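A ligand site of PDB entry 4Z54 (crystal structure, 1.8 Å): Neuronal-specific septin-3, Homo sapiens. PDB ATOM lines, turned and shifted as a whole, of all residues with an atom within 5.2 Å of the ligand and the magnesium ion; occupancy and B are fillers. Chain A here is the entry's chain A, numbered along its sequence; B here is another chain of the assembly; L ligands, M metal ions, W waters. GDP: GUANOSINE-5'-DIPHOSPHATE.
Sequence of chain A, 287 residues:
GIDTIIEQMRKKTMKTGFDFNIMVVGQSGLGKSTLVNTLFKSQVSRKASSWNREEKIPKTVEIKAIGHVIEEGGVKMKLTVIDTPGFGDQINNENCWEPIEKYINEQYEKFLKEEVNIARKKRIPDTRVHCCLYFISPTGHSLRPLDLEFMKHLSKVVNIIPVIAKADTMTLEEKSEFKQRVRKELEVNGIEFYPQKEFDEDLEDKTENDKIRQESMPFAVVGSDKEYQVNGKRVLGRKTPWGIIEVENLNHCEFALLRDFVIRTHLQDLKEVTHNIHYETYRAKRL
N of Ser 33 sits at hydrogen-bond distance from O2A of the ligand, at 3.4 Å. The side-chain carboxylate (OE2) of Glu 174 of chain B is in hydrogen-bond range of an oxygen (O2') of the ligand (2.6 Å). The backbone NH of Thr 34 lies within hydrogen-bond range of an oxygen (O2A) of the ligand, 2.8 Å away. OG1 of Thr 34 lies within hydrogen-bond range of O2A of the ligand, 2.6 Å away. O3B of the ligand lies within hydrogen-bond range of N of Lys 32. NZ of Lys 32 is in salt-bridge range of O3B of the ligand, at 2.7 Å. A nitrogen (N1) of the ligand is in hydrogen-bond range of the side-chain carboxylate (OD1) of Asp 168 (2.8 Å). The backbone NH (N) of Gly 29 sits at hydrogen-bond distance from an oxygen (O1B) of the ligand. The backbone NH (N) of Gly 223 sits at hydrogen-bond distance from an oxygen (O6) of the ligand, at 2.8 Å. O of Thr 169 of chain B lies within hydrogen-bond range of N2 of the ligand (2.9 Å). The backbone NH of Gly 31 sits at hydrogen-bond distance from an oxygen (O3A) of the ligand (2.9 Å). An oxygen (O1B) of the ligand lies within hydrogen-bond range of a ring nitrogen (NE2) of His 141 of chain B. The backbone NH (N) of Leu 30 lies within hydrogen-bond range of an oxygen (O3B) of the ligand, at 3.1 Å. NH1 of Arg 238 sits close to N3 of the ligand (3.5 Å).
OE1 of Glu 174 of chain B is in salt-bridge range of NH2 of Arg 238. The side-chain amino group (NZ) of Lys 32 sits at hydrogen-bond distance from the backbone carbonyl oxygen (O) of Gln 27, 3.1 Å away. OD2 of Asp 168 is in salt-bridge range of NE of Arg 238 (3.97 Å). O of Gly 29 lies within hydrogen-bond range of NZ of Lys 166 (2.8 Å). The guanidinium group (NH2) of Arg 238 lies within hydrogen-bond range of the backbone carbonyl oxygen (O) of Thr 169 of chain B (3.0 Å). The backbone NH (N) of His 141 of chain B lies close to the side-chain hydroxyl (OG1) of Thr 139 of chain B (3.2 Å). The backbone NH (N) of Lys 166 sits at hydrogen-bond distance from the backbone carbonyl oxygen (O) of Val 221 (3.5 Å). The side-chain hydroxyl (OG1) of Thr 169 of chain A is in hydrogen-bond range of the backbone carbonyl oxygen (O) of Lys 166, 2.8 Å away.
O of Gln 27 touches O3B of the ligand, at 3.999 Å. Ser 28 touches the ligand. Lys 56 touches the ligand. Lys 166 touches the ligand. CA of Val 222 touches O6 of the ligand, at 3.3 Å. Thr 139 of chain B touches the ligand (O to C5', 3.3 Å). Hydrophobic or aromatic side chains within 4 Å of the ligand: Val 222 and His 141 of chain B. The nearest printed residue that does not touch the ligand is Thr 60 (4.04 Å).
The nearest printed residue that does not touch the magnesium ion is Asp 83 (4.02 Å).
O2B of the ligand is bound to the magnesium ion (2.0 Å). Water W4 binds the magnesium ion. OG1 of Thr 60 binds the magnesium ion, at 2.1 Å. Water W1 is bound to the magnesium ion (2.1 Å). OG of Ser 33 binds the magnesium ion. The magnesium ion is bound by water W2 (2.1 Å).
Water W2 bridges the backbone carbonyl oxygen (O) of Pro 58 and an oxygen (O1A) of the ligand. Water W4 bridges O1B of the ligand (2.8 Å) and N of Thr 60 (2.9 Å). Water W7 lies within hydrogen-bond range of an oxygen (O1A) of the ligand (2.7 Å), the backbone carbonyl oxygen (O) of Ile 57 (2.7 Å) and the side-chain amino group (NZ) of Lys 56 (2.9 Å). Water W9 lies within hydrogen-bond range of the backbone carbonyl oxygen (O) of Gly 31, a nitrogen (N7) of the ligand and the backbone NH (N) of Gly 223. Water W5 lies within hydrogen-bond range of the side-chain carboxylate of Glu 174 of chain B (2.6 Å) and an oxygen (O2') of the ligand (3.2 Å). Water W10 lies within hydrogen-bond range of NH1 of Arg 238, O of Gly 223 and N7 of the ligand.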
ATOM      1  N   GLN A  27      -7.871  21.539 -28.827  1.00  0.00           N
ATOM      2  CA  GLN A  27      -8.093  22.854 -28.251  1.00  0.00           C
ATOM      3  C   GLN A  27      -9.420  22.913 -27.510  1.00  0.00           C
ATOM      4  O   GLN A  27     -10.302  22.085 -27.728  1.00  0.00           O
ATOM      5  CB  GLN A  27      -8.007  23.915 -29.340  1.00  0.00           C
ATOM      6  CG  GLN A  27      -6.706  23.787 -30.115  1.00  0.00           C
ATOM      7  CD  GLN A  27      -6.371  24.993 -30.955  1.00  0.00           C
ATOM      8  OE1 GLN A  27      -6.897  26.076 -30.726  1.00  0.00           O
ATOM      9  NE2 GLN A  27      -5.501  24.803 -31.934  1.00  0.00           N
ATOM     10  N   SER A  28      -9.560  23.880 -26.600  1.00  0.00           N
ATOM     11  CA  SER A  28     -10.776  23.975 -25.815  1.00  0.00           C
ATOM     12  C   SER A  28     -11.940  24.398 -26.689  1.00  0.00           C
ATOM     13  O   SER A  28     -11.755  25.132 -27.663  1.00  0.00           O
ATOM     14  CB  SER A  28     -10.615  24.966 -24.650  1.00  0.00           C
ATOM     15  OG  SER A  28      -9.848  24.382 -23.604  1.00  0.00           O
ATOM     16  N   GLY A  29     -13.132  23.940 -26.329  1.00  0.00           N
ATOM     17  CA  GLY A  29     -14.344  24.354 -27.010  1.00  0.00           C
ATOM     18  C   GLY A  29     -14.684  23.509 -28.227  1.00  0.00           C
ATOM     19  O   GLY A  29     -15.443  23.951 -29.087  1.00  0.00           O
ATOM     20  N   LEU A  30     -14.116  22.307 -28.306  1.00  0.00           N
ATOM     21  CA  LEU A  30     -14.315  21.456 -29.478  1.00  0.00           C
ATOM     22  C   LEU A  30     -15.273  20.306 -29.206  1.00  0.00           C
ATOM     23  O   LEU A  30     -15.564  19.501 -30.091  1.00  0.00           O
ATOM     24  CB  LEU A  30     -12.956  20.908 -29.974  1.00  0.00           C
ATOM     25  CG  LEU A  30     -12.099  21.948 -30.719  1.00  0.00           C
ATOM     26  CD1 LEU A  30     -10.823  21.332 -31.315  1.00  0.00           C
ATOM     27  CD2 LEU A  30     -12.923  22.609 -31.801  1.00  0.00           C
ATOM     28  N   GLY A  31     -15.793  20.242 -27.984  1.00  0.00           N
ATOM     29  CA  GLY A  31     -16.765  19.204 -27.640  1.00  0.00           C
ATOM     30  C   GLY A  31     -16.123  17.966 -27.044  1.00  0.00           C
ATOM     31  O   GLY A  31     -16.744  16.896 -27.000  1.00  0.00           O
ATOM     32  N   LYS A  32     -14.882  18.104 -26.577  1.00  0.00           N
ATOM     33  CA  LYS A  32     -14.148  16.946 -26.060  1.00  0.00           C
ATOM     34  C   LYS A  32     -14.825  16.305 -24.848  1.00  0.00           C
ATOM     35  O   LYS A  32     -15.041  15.074 -24.810  1.00  0.00           O
ATOM     36  CB  LYS A  32     -12.698  17.333 -25.738  1.00  0.00           C
ATOM     37  CG  LYS A  32     -11.911  17.772 -26.989  1.00  0.00           C
ATOM     38  CD  LYS A  32     -10.401  17.984 -26.719  1.00  0.00           C
ATOM     39  CE  LYS A  32     -10.153  18.738 -25.414  1.00  0.00           C
ATOM     40  NZ  LYS A  32     -10.825  20.106 -25.436  1.00  0.00           N
ATOM     41  N   SER A  33     -15.177  17.133 -23.865  1.00  0.00           N
ATOM     42  CA  SER A  33     -15.705  16.644 -22.599  1.00  0.00           C
ATOM     43  C   SER A  33     -17.113  16.104 -22.821  1.00  0.00           C
ATOM     44  O   SER A  33     -17.534  15.128 -22.203  1.00  0.00           O
ATOM     45  CB  SER A  33     -15.709  17.753 -21.539  1.00  0.00           C
ATOM     46  OG  SER A  33     -14.391  18.067 -21.103  1.00  0.00           O
ATOM     47  N   THR A  34     -17.839  16.753 -23.722  1.00  0.00           N
ATOM     48  CA  THR A  34     -19.143  16.286 -24.143  1.00  0.00           C
ATOM     49  C   THR A  34     -19.047  14.879 -24.766  1.00  0.00           C
ATOM     50  O   THR A  34     -19.837  13.990 -24.418  1.00  0.00           O
ATOM     51  CB  THR A  34     -19.788  17.256 -25.172  1.00  0.00           C
ATOM     52  OG1 THR A  34     -19.999  18.539 -24.559  1.00  0.00           O
ATOM     53  CG2 THR A  34     -21.119  16.703 -25.653  1.00  0.00           C
ATOM     54  N   LEU A  35     -18.066  14.678 -25.649  1.00  0.00           N
ATOM     55  CA  LEU A  35     -17.912  13.369 -26.297  1.00  0.00           C
ATOM     56  C   LEU A  35     -17.492  12.274 -25.317  1.00  0.00           C
ATOM     57  O   LEU A  35     -17.886  11.115 -25.465  1.00  0.00           O
ATOM     58  CB  LEU A  35     -16.909  13.447 -27.452  1.00  0.00           C
ATOM     59  CG  LEU A  35     -17.151  12.297 -28.448  1.00  0.00           C
ATOM     60  CD1 LEU A  35     -18.246  12.670 -29.460  1.00  0.00           C
ATOM     61  CD2 LEU A  35     -15.879  11.879 -29.142  1.00  0.00           C
ATOM     62  N   LYS A  56     -24.016  23.319 -17.651  1.00  0.00           N
ATOM     63  CA  LYS A  56     -23.011  23.246 -18.646  1.00  0.00           C
ATOM     64  C   LYS A  56     -21.805  22.479 -18.131  1.00  0.00           C
ATOM     65  O   LYS A  56     -21.496  22.545 -16.989  1.00  0.00           O
ATOM     66  CB  LYS A  56     -22.621  24.651 -18.972  1.00  0.00           C
ATOM     67  CG  LYS A  56     -21.704  24.788 -20.122  1.00  0.00           C
ATOM     68  CD  LYS A  56     -21.081  26.164 -20.156  1.00  0.00           C
ATOM     69  CE  LYS A  56     -20.744  26.520 -21.603  1.00  0.00           C
ATOM     70  NZ  LYS A  56     -19.728  25.632 -22.249  1.00  0.00           N
ATOM     71  N   ILE A  57     -21.148  21.721 -18.979  1.00  0.00           N
ATOM     72  CA  ILE A  57     -19.894  21.085 -18.574  1.00  0.00           C
ATOM     73  C   ILE A  57     -18.829  22.172 -18.386  1.00  0.00           C
ATOM     74  O   ILE A  57     -18.588  22.976 -19.287  1.00  0.00           O
ATOM     75  CB  ILE A  57     -19.414  20.051 -19.598  1.00  0.00           C
ATOM     76  CG1 ILE A  57     -20.491  18.977 -19.802  1.00  0.00           C
ATOM     77  CG2 ILE A  57     -18.078  19.413 -19.146  1.00  0.00           C
ATOM     78  CD1 ILE A  57     -20.232  18.089 -20.983  1.00  0.00           C
ATOM     79  N   PRO A  58     -18.193  22.221 -17.199  1.00  0.00           N
ATOM     80  CA  PRO A  58     -17.143  23.215 -16.972  1.00  0.00           C
ATOM     81  C   PRO A  58     -15.960  23.042 -17.922  1.00  0.00           C
ATOM     82  O   PRO A  58     -15.720  21.956 -18.453  1.00  0.00           O
ATOM     83  CB  PRO A  58     -16.706  22.952 -15.525  1.00  0.00           C
ATOM     84  CG  PRO A  58     -17.826  22.205 -14.901  1.00  0.00           C
ATOM     85  CD  PRO A  58     -18.419  21.383 -16.005  1.00  0.00           C
ATOM     86  N   LYS A  59     -15.236  24.121 -18.138  1.00  0.00           N
ATOM     87  CA  LYS A  59     -13.996  24.044 -18.895  1.00  0.00           C
ATOM     88  C   LYS A  59     -13.054  23.079 -18.182  1.00  0.00           C
ATOM     89  O   LYS A  59     -12.967  23.087 -16.953  1.00  0.00           O
ATOM     90  CB  LYS A  59     -13.365  25.438 -19.027  1.00  0.00           C
ATOM     91  CG  LYS A  59     -12.071  25.449 -19.791  1.00  0.00           C
ATOM     92  CD  LYS A  59     -11.515  26.850 -19.965  1.00  0.00           C
ATOM     93  CE  LYS A  59     -10.194  26.805 -20.731  1.00  0.00           C
ATOM     94  NZ  LYS A  59      -9.630  28.161 -20.975  1.00  0.00           N
ATOM     95  N   THR A  60     -12.389  22.228 -18.943  1.00  0.00           N
ATOM     96  CA  THR A  60     -11.507  21.222 -18.371  1.00  0.00           C
ATOM     97  C   THR A  60     -10.140  21.842 -18.106  1.00  0.00           C
ATOM     98  O   THR A  60      -9.472  22.298 -19.019  1.00  0.00           O
ATOM     99  CB  THR A  60     -11.378  20.022 -19.312  1.00  0.00           C
ATOM    100  OG1 THR A  60     -12.694  19.678 -19.785  1.00  0.00           O
ATOM    101  CG2 THR A  60     -10.757  18.802 -18.576  1.00  0.00           C
ATOM    102  N   ASP A  83      -9.820  12.895 -19.891  1.00  0.00           N
ATOM    103  CA  ASP A  83     -10.176  14.222 -20.384  1.00  0.00           C
ATOM    104  C   ASP A  83      -8.985  15.114 -20.075  1.00  0.00           C
ATOM    105  O   ASP A  83      -8.279  14.904 -19.082  1.00  0.00           O
ATOM    106  CB  ASP A  83     -11.447  14.731 -19.703  1.00  0.00           C
ATOM    107  CG  ASP A  83     -12.171  15.808 -20.512  1.00  0.00           C
ATOM    108  OD1 ASP A  83     -11.641  16.252 -21.562  1.00  0.00           O
ATOM    109  OD2 ASP A  83     -13.264  16.215 -20.063  1.00  0.00           O
ATOM    110  N   THR A  84      -8.739  16.078 -20.944  1.00  0.00           N
ATOM    111  CA  THR A  84      -7.527  16.892 -20.840  1.00  0.00           C
ATOM    112  C   THR A  84      -7.848  18.367 -21.055  1.00  0.00           C
ATOM    113  O   THR A  84      -8.791  18.689 -21.778  1.00  0.00           O
ATOM    114  CB  THR A  84      -6.468  16.454 -21.889  1.00  0.00           C
ATOM    115  OG1 THR A  84      -6.987  16.689 -23.199  1.00  0.00           O
ATOM    116  CG2 THR A  84      -6.124  14.963 -21.755  1.00  0.00           C
ATOM    117  N   LYS A 166     -17.435  18.746 -33.822  1.00  0.00           N
ATOM    118  CA  LYS A 166     -18.620  19.539 -34.161  1.00  0.00           C
ATOM    119  C   LYS A 166     -18.951  19.468 -35.651  1.00  0.00           C
ATOM    120  O   LYS A 166     -19.079  20.491 -36.300  1.00  0.00           O
ATOM    121  CB  LYS A 166     -18.420  21.000 -33.780  1.00  0.00           C
ATOM    122  CG  LYS A 166     -18.074  21.236 -32.323  1.00  0.00           C
ATOM    123  CD  LYS A 166     -18.104  22.718 -32.013  1.00  0.00           C
ATOM    124  CE  LYS A 166     -18.051  22.981 -30.534  1.00  0.00           C
ATOM    125  NZ  LYS A 166     -17.921  24.444 -30.239  1.00  0.00           N
ATOM    126  N   ALA A 167     -19.075  18.263 -36.170  1.00  0.00           N
ATOM    127  CA  ALA A 167     -19.203  18.094 -37.612  1.00  0.00           C
ATOM    128  C   ALA A 167     -20.526  18.625 -38.160  1.00  0.00           C
ATOM    129  O   ALA A 167     -20.670  18.800 -39.368  1.00  0.00           O
ATOM    130  CB  ALA A 167     -19.024  16.635 -37.985  1.00  0.00           C
ATOM    131  N   ASP A 168     -21.478  18.901 -37.275  1.00  0.00           N
ATOM    132  CA  ASP A 168     -22.752  19.462 -37.654  1.00  0.00           C
ATOM    133  C   ASP A 168     -22.545  20.892 -38.150  1.00  0.00           C
ATOM    134  O   ASP A 168     -23.433  21.466 -38.759  1.00  0.00           O
ATOM    135  CB  ASP A 168     -23.722  19.453 -36.474  1.00  0.00           C
ATOM    136  CG  ASP A 168     -23.124  20.130 -35.243  1.00  0.00           C
ATOM    137  OD1 ASP A 168     -22.041  19.722 -34.796  1.00  0.00           O
ATOM    138  OD2 ASP A 168     -23.746  21.082 -34.724  1.00  0.00           O
ATOM    139  N   THR A 169     -21.353  21.430 -37.866  1.00  0.00           N
ATOM    140  CA  THR A 169     -20.897  22.745 -38.349  1.00  0.00           C
ATOM    141  C   THR A 169     -20.821  22.802 -39.859  1.00  0.00           C
ATOM    142  O   THR A 169     -20.865  23.883 -40.466  1.00  0.00           O
ATOM    143  CB  THR A 169     -19.456  23.098 -37.781  1.00  0.00           C
ATOM    144  OG1 THR A 169     -19.510  23.218 -36.367  1.00  0.00           O
ATOM    145  CG2 THR A 169     -18.921  24.416 -38.345  1.00  0.00           C
ATOM    146  N   VAL A 221     -17.522  13.797 -36.164  1.00  0.00           N
ATOM    147  CA  VAL A 221     -18.421  13.431 -35.096  1.00  0.00           C
ATOM    148  C   VAL A 221     -19.274  14.593 -34.572  1.00  0.00           C
ATOM    149  O   VAL A 221     -18.940  15.769 -34.734  1.00  0.00           O
ATOM    150  CB  VAL A 221     -17.666  12.803 -33.899  1.00  0.00           C
ATOM    151  CG1 VAL A 221     -16.742  11.687 -34.390  1.00  0.00           C
ATOM    152  CG2 VAL A 221     -16.882  13.854 -33.148  1.00  0.00           C
ATOM    153  N   VAL A 222     -20.380  14.222 -33.969  1.00  0.00           N
ATOM    154  CA  VAL A 222     -21.200  15.158 -33.230  1.00  0.00           C
ATOM    155  C   VAL A 222     -21.344  14.545 -31.850  1.00  0.00           C
ATOM    156  O   VAL A 222     -21.546  13.350 -31.743  1.00  0.00           O
ATOM    157  CB  VAL A 222     -22.575  15.388 -33.908  1.00  0.00           C
ATOM    158  CG1 VAL A 222     -23.556  16.104 -32.960  1.00  0.00           C
ATOM    159  CG2 VAL A 222     -22.400  16.159 -35.230  1.00  0.00           C
ATOM    160  N   GLY A 223     -21.175  15.340 -30.805  1.00  0.00           N
ATOM    161  CA  GLY A 223     -21.299  14.812 -29.463  1.00  0.00           C
ATOM    162  C   GLY A 223     -22.526  15.351 -28.754  1.00  0.00           C
ATOM    163  O   GLY A 223     -22.929  16.489 -28.970  1.00  0.00           O
ATOM    164  N   ARG A 238     -28.397  16.480 -30.408  1.00  0.00           N
ATOM    165  CA  ARG A 238     -28.368  17.916 -30.140  1.00  0.00           C
ATOM    166  C   ARG A 238     -29.633  18.533 -30.657  1.00  0.00           C
ATOM    167  O   ARG A 238     -29.969  18.352 -31.826  1.00  0.00           O
ATOM    168  CB  ARG A 238     -27.153  18.589 -30.811  1.00  0.00           C
ATOM    169  CG  ARG A 238     -25.904  18.537 -30.001  1.00  0.00           C
ATOM    170  CD  ARG A 238     -24.739  19.168 -30.739  1.00  0.00           C
ATOM    171  NE  ARG A 238     -24.888  20.611 -30.952  1.00  0.00           N
ATOM    172  CZ  ARG A 238     -24.735  21.529 -29.996  1.00  0.00           C
ATOM    173  NH1 ARG A 238     -24.459  21.146 -28.746  1.00  0.00           N
ATOM    174  NH2 ARG A 238     -24.858  22.830 -30.289  1.00  0.00           N
ATOM    175  N   THR B 139     -16.881  28.862 -28.508  1.00  0.00           N
ATOM    176  CA  THR B 139     -16.383  27.722 -27.730  1.00  0.00           C
ATOM    177  C   THR B 139     -17.240  27.337 -26.536  1.00  0.00           C
ATOM    178  O   THR B 139     -17.130  26.227 -26.022  1.00  0.00           O
ATOM    179  CB  THR B 139     -14.999  28.029 -27.176  1.00  0.00           C
ATOM    180  OG1 THR B 139     -15.082  29.222 -26.384  1.00  0.00           O
ATOM    181  CG2 THR B 139     -14.010  28.231 -28.314  1.00  0.00           C
ATOM    182  N   GLY B 140     -18.063  28.265 -26.042  1.00  0.00           N
ATOM    183  CA  GLY B 140     -18.814  28.011 -24.832  1.00  0.00           C
ATOM    184  C   GLY B 140     -18.039  28.354 -23.558  1.00  0.00           C
ATOM    185  O   GLY B 140     -18.601  28.355 -22.469  1.00  0.00           O
ATOM    186  N   HIS B 141     -16.755  28.664 -23.708  1.00  0.00           N
ATOM    187  CA  HIS B 141     -15.890  28.872 -22.536  1.00  0.00           C
ATOM    188  C   HIS B 141     -15.368  30.299 -22.449  1.00  0.00           C
ATOM    189  O   HIS B 141     -15.712  31.133 -23.263  1.00  0.00           O
ATOM    190  CB  HIS B 141     -14.712  27.915 -22.565  1.00  0.00           C
ATOM    191  CG  HIS B 141     -15.112  26.471 -22.503  1.00  0.00           C
ATOM    192  ND1 HIS B 141     -15.948  25.981 -21.528  1.00  0.00           N
ATOM    193  CD2 HIS B 141     -14.768  25.416 -23.272  1.00  0.00           C
ATOM    194  CE1 HIS B 141     -16.120  24.684 -21.702  1.00  0.00           C
ATOM    195  NE2 HIS B 141     -15.410  24.319 -22.757  1.00  0.00           N
ATOM    196  N   THR B 169     -23.558  27.152 -34.867  1.00  0.00           N
ATOM    197  CA  THR B 169     -22.868  26.168 -34.021  1.00  0.00           C
ATOM    198  C   THR B 169     -23.586  25.922 -32.700  1.00  0.00           C
ATOM    199  O   THR B 169     -23.520  24.833 -32.139  1.00  0.00           O
ATOM    200  CB  THR B 169     -21.427  26.654 -33.705  1.00  0.00           C
ATOM    201  OG1 THR B 169     -20.681  26.763 -34.921  1.00  0.00           O
ATOM    202  CG2 THR B 169     -20.682  25.729 -32.730  1.00  0.00           C
ATOM    203  N   MET B 170     -24.292  26.935 -32.223  1.00  0.00           N
ATOM    204  CA  MET B 170     -24.835  26.922 -30.869  1.00  0.00           C
ATOM    205  C   MET B 170     -26.331  26.684 -30.810  1.00  0.00           C
ATOM    206  O   MET B 170     -27.073  27.176 -31.643  1.00  0.00           O
ATOM    207  CB  MET B 170     -24.517  28.247 -30.181  1.00  0.00           C
ATOM    208  CG  MET B 170     -23.030  28.496 -30.002  1.00  0.00           C
ATOM    209  SD  MET B 170     -22.693  30.153 -29.338  1.00  0.00           S
ATOM    210  CE  MET B 170     -23.160  31.183 -30.710  1.00  0.00           C
ATOM    211  N   GLU B 174     -27.141  27.719 -25.537  1.00  0.00           N
ATOM    212  CA  GLU B 174     -25.687  27.902 -25.580  1.00  0.00           C
ATOM    213  C   GLU B 174     -25.345  29.326 -26.023  1.00  0.00           C
ATOM    214  O   GLU B 174     -24.394  29.924 -25.535  1.00  0.00           O
ATOM    215  CB  GLU B 174     -25.040  26.896 -26.529  1.00  0.00           C
ATOM    216  CG  GLU B 174     -25.000  25.472 -25.995  1.00  0.00           C
ATOM    217  CD  GLU B 174     -24.615  24.434 -27.062  1.00  0.00           C
ATOM    218  OE1 GLU B 174     -24.484  24.812 -28.254  1.00  0.00           O
ATOM    219  OE2 GLU B 174     -24.443  23.243 -26.706  1.00  0.00           O
HETATM  220  PB  GDP L   1     -14.237  20.941 -24.623  1.00  0.00           P
HETATM  221  O1B GDP L   1     -13.772  22.289 -24.103  1.00  0.00           O
HETATM  222  O2B GDP L   1     -14.236  19.897 -23.517  1.00  0.00           O
HETATM  223  O3B GDP L   1     -13.478  20.543 -25.849  1.00  0.00           O
HETATM  224  O3A GDP L   1     -15.750  21.107 -25.189  1.00  0.00           O
HETATM  225  PA  GDP L   1     -17.080  20.926 -24.313  1.00  0.00           P
HETATM  226  O1A GDP L   1     -17.002  21.626 -22.983  1.00  0.00           O
HETATM  227  O2A GDP L   1     -17.563  19.490 -24.217  1.00  0.00           O
HETATM  228  O5' GDP L   1     -18.161  21.681 -25.267  1.00  0.00           O
HETATM  229  C5' GDP L   1     -17.978  23.061 -25.608  1.00  0.00           C
HETATM  230  C4' GDP L   1     -19.269  23.568 -26.245  1.00  0.00           C
HETATM  231  O4' GDP L   1     -19.523  22.863 -27.468  1.00  0.00           O
HETATM  232  C3' GDP L   1     -20.479  23.291 -25.368  1.00  0.00           C
HETATM  233  O3' GDP L   1     -21.389  24.381 -25.577  1.00  0.00           O
HETATM  234  C2' GDP L   1     -21.083  22.049 -25.956  1.00  0.00           C
HETATM  235  O2' GDP L   1     -22.489  21.943 -25.624  1.00  0.00           O
HETATM  236  C1' GDP L   1     -20.825  22.263 -27.428  1.00  0.00           C
HETATM  237  N9  GDP L   1     -20.751  21.004 -28.175  1.00  0.00           N
HETATM  238  C8  GDP L   1     -20.321  19.787 -27.744  1.00  0.00           C
HETATM  239  N7  GDP L   1     -20.360  18.887 -28.749  1.00  0.00           N
HETATM  240  C5  GDP L   1     -20.788  19.541 -29.861  1.00  0.00           C
HETATM  241  C6  GDP L   1     -21.053  19.185 -31.273  1.00  0.00           C
HETATM  242  O6  GDP L   1     -20.860  18.023 -31.711  1.00  0.00           O
HETATM  243  N1  GDP L   1     -21.503  20.143 -32.100  1.00  0.00           N
HETATM  244  C2  GDP L   1     -21.676  21.407 -31.675  1.00  0.00           C
HETATM  245  N2  GDP L   1     -22.109  22.312 -32.579  1.00  0.00           N
HETATM  246  N3  GDP L   1     -21.468  21.808 -30.394  1.00  0.00           N
HETATM  247  C4  GDP L   1     -21.030  20.921 -29.474  1.00  0.00           C
HETATM  248 MG    MG M   1     -13.482  19.896 -21.667  1.00  0.00          MG
HETATM  249  O   HOH W   1     -11.814  18.813 -22.366  1.00  0.00           O
HETATM  250  O   HOH W   2     -15.184  20.968 -20.988  1.00  0.00           O
HETATM  251  O   HOH W   3     -22.307  19.777 -23.757  1.00  0.00           O
HETATM  252  O   HOH W   4     -12.432  21.631 -21.790  1.00  0.00           O
HETATM  253  O   HOH W   5     -25.547  21.966 -24.740  1.00  0.00           O
HETATM  254  O   HOH W   6     -21.667  24.602 -29.652  1.00  0.00           O
HETATM  255  O   HOH W   7     -19.115  22.851 -21.934  1.00  0.00           O
HETATM  256  O   HOH W   8     -23.125  24.028 -23.089  1.00  0.00           O
HETATM  257  O   HOH W   9     -18.677  16.636 -28.960  1.00  0.00           O
HETATM  258  O   HOH W  10     -23.627  18.786 -27.685  1.00  0.00           O
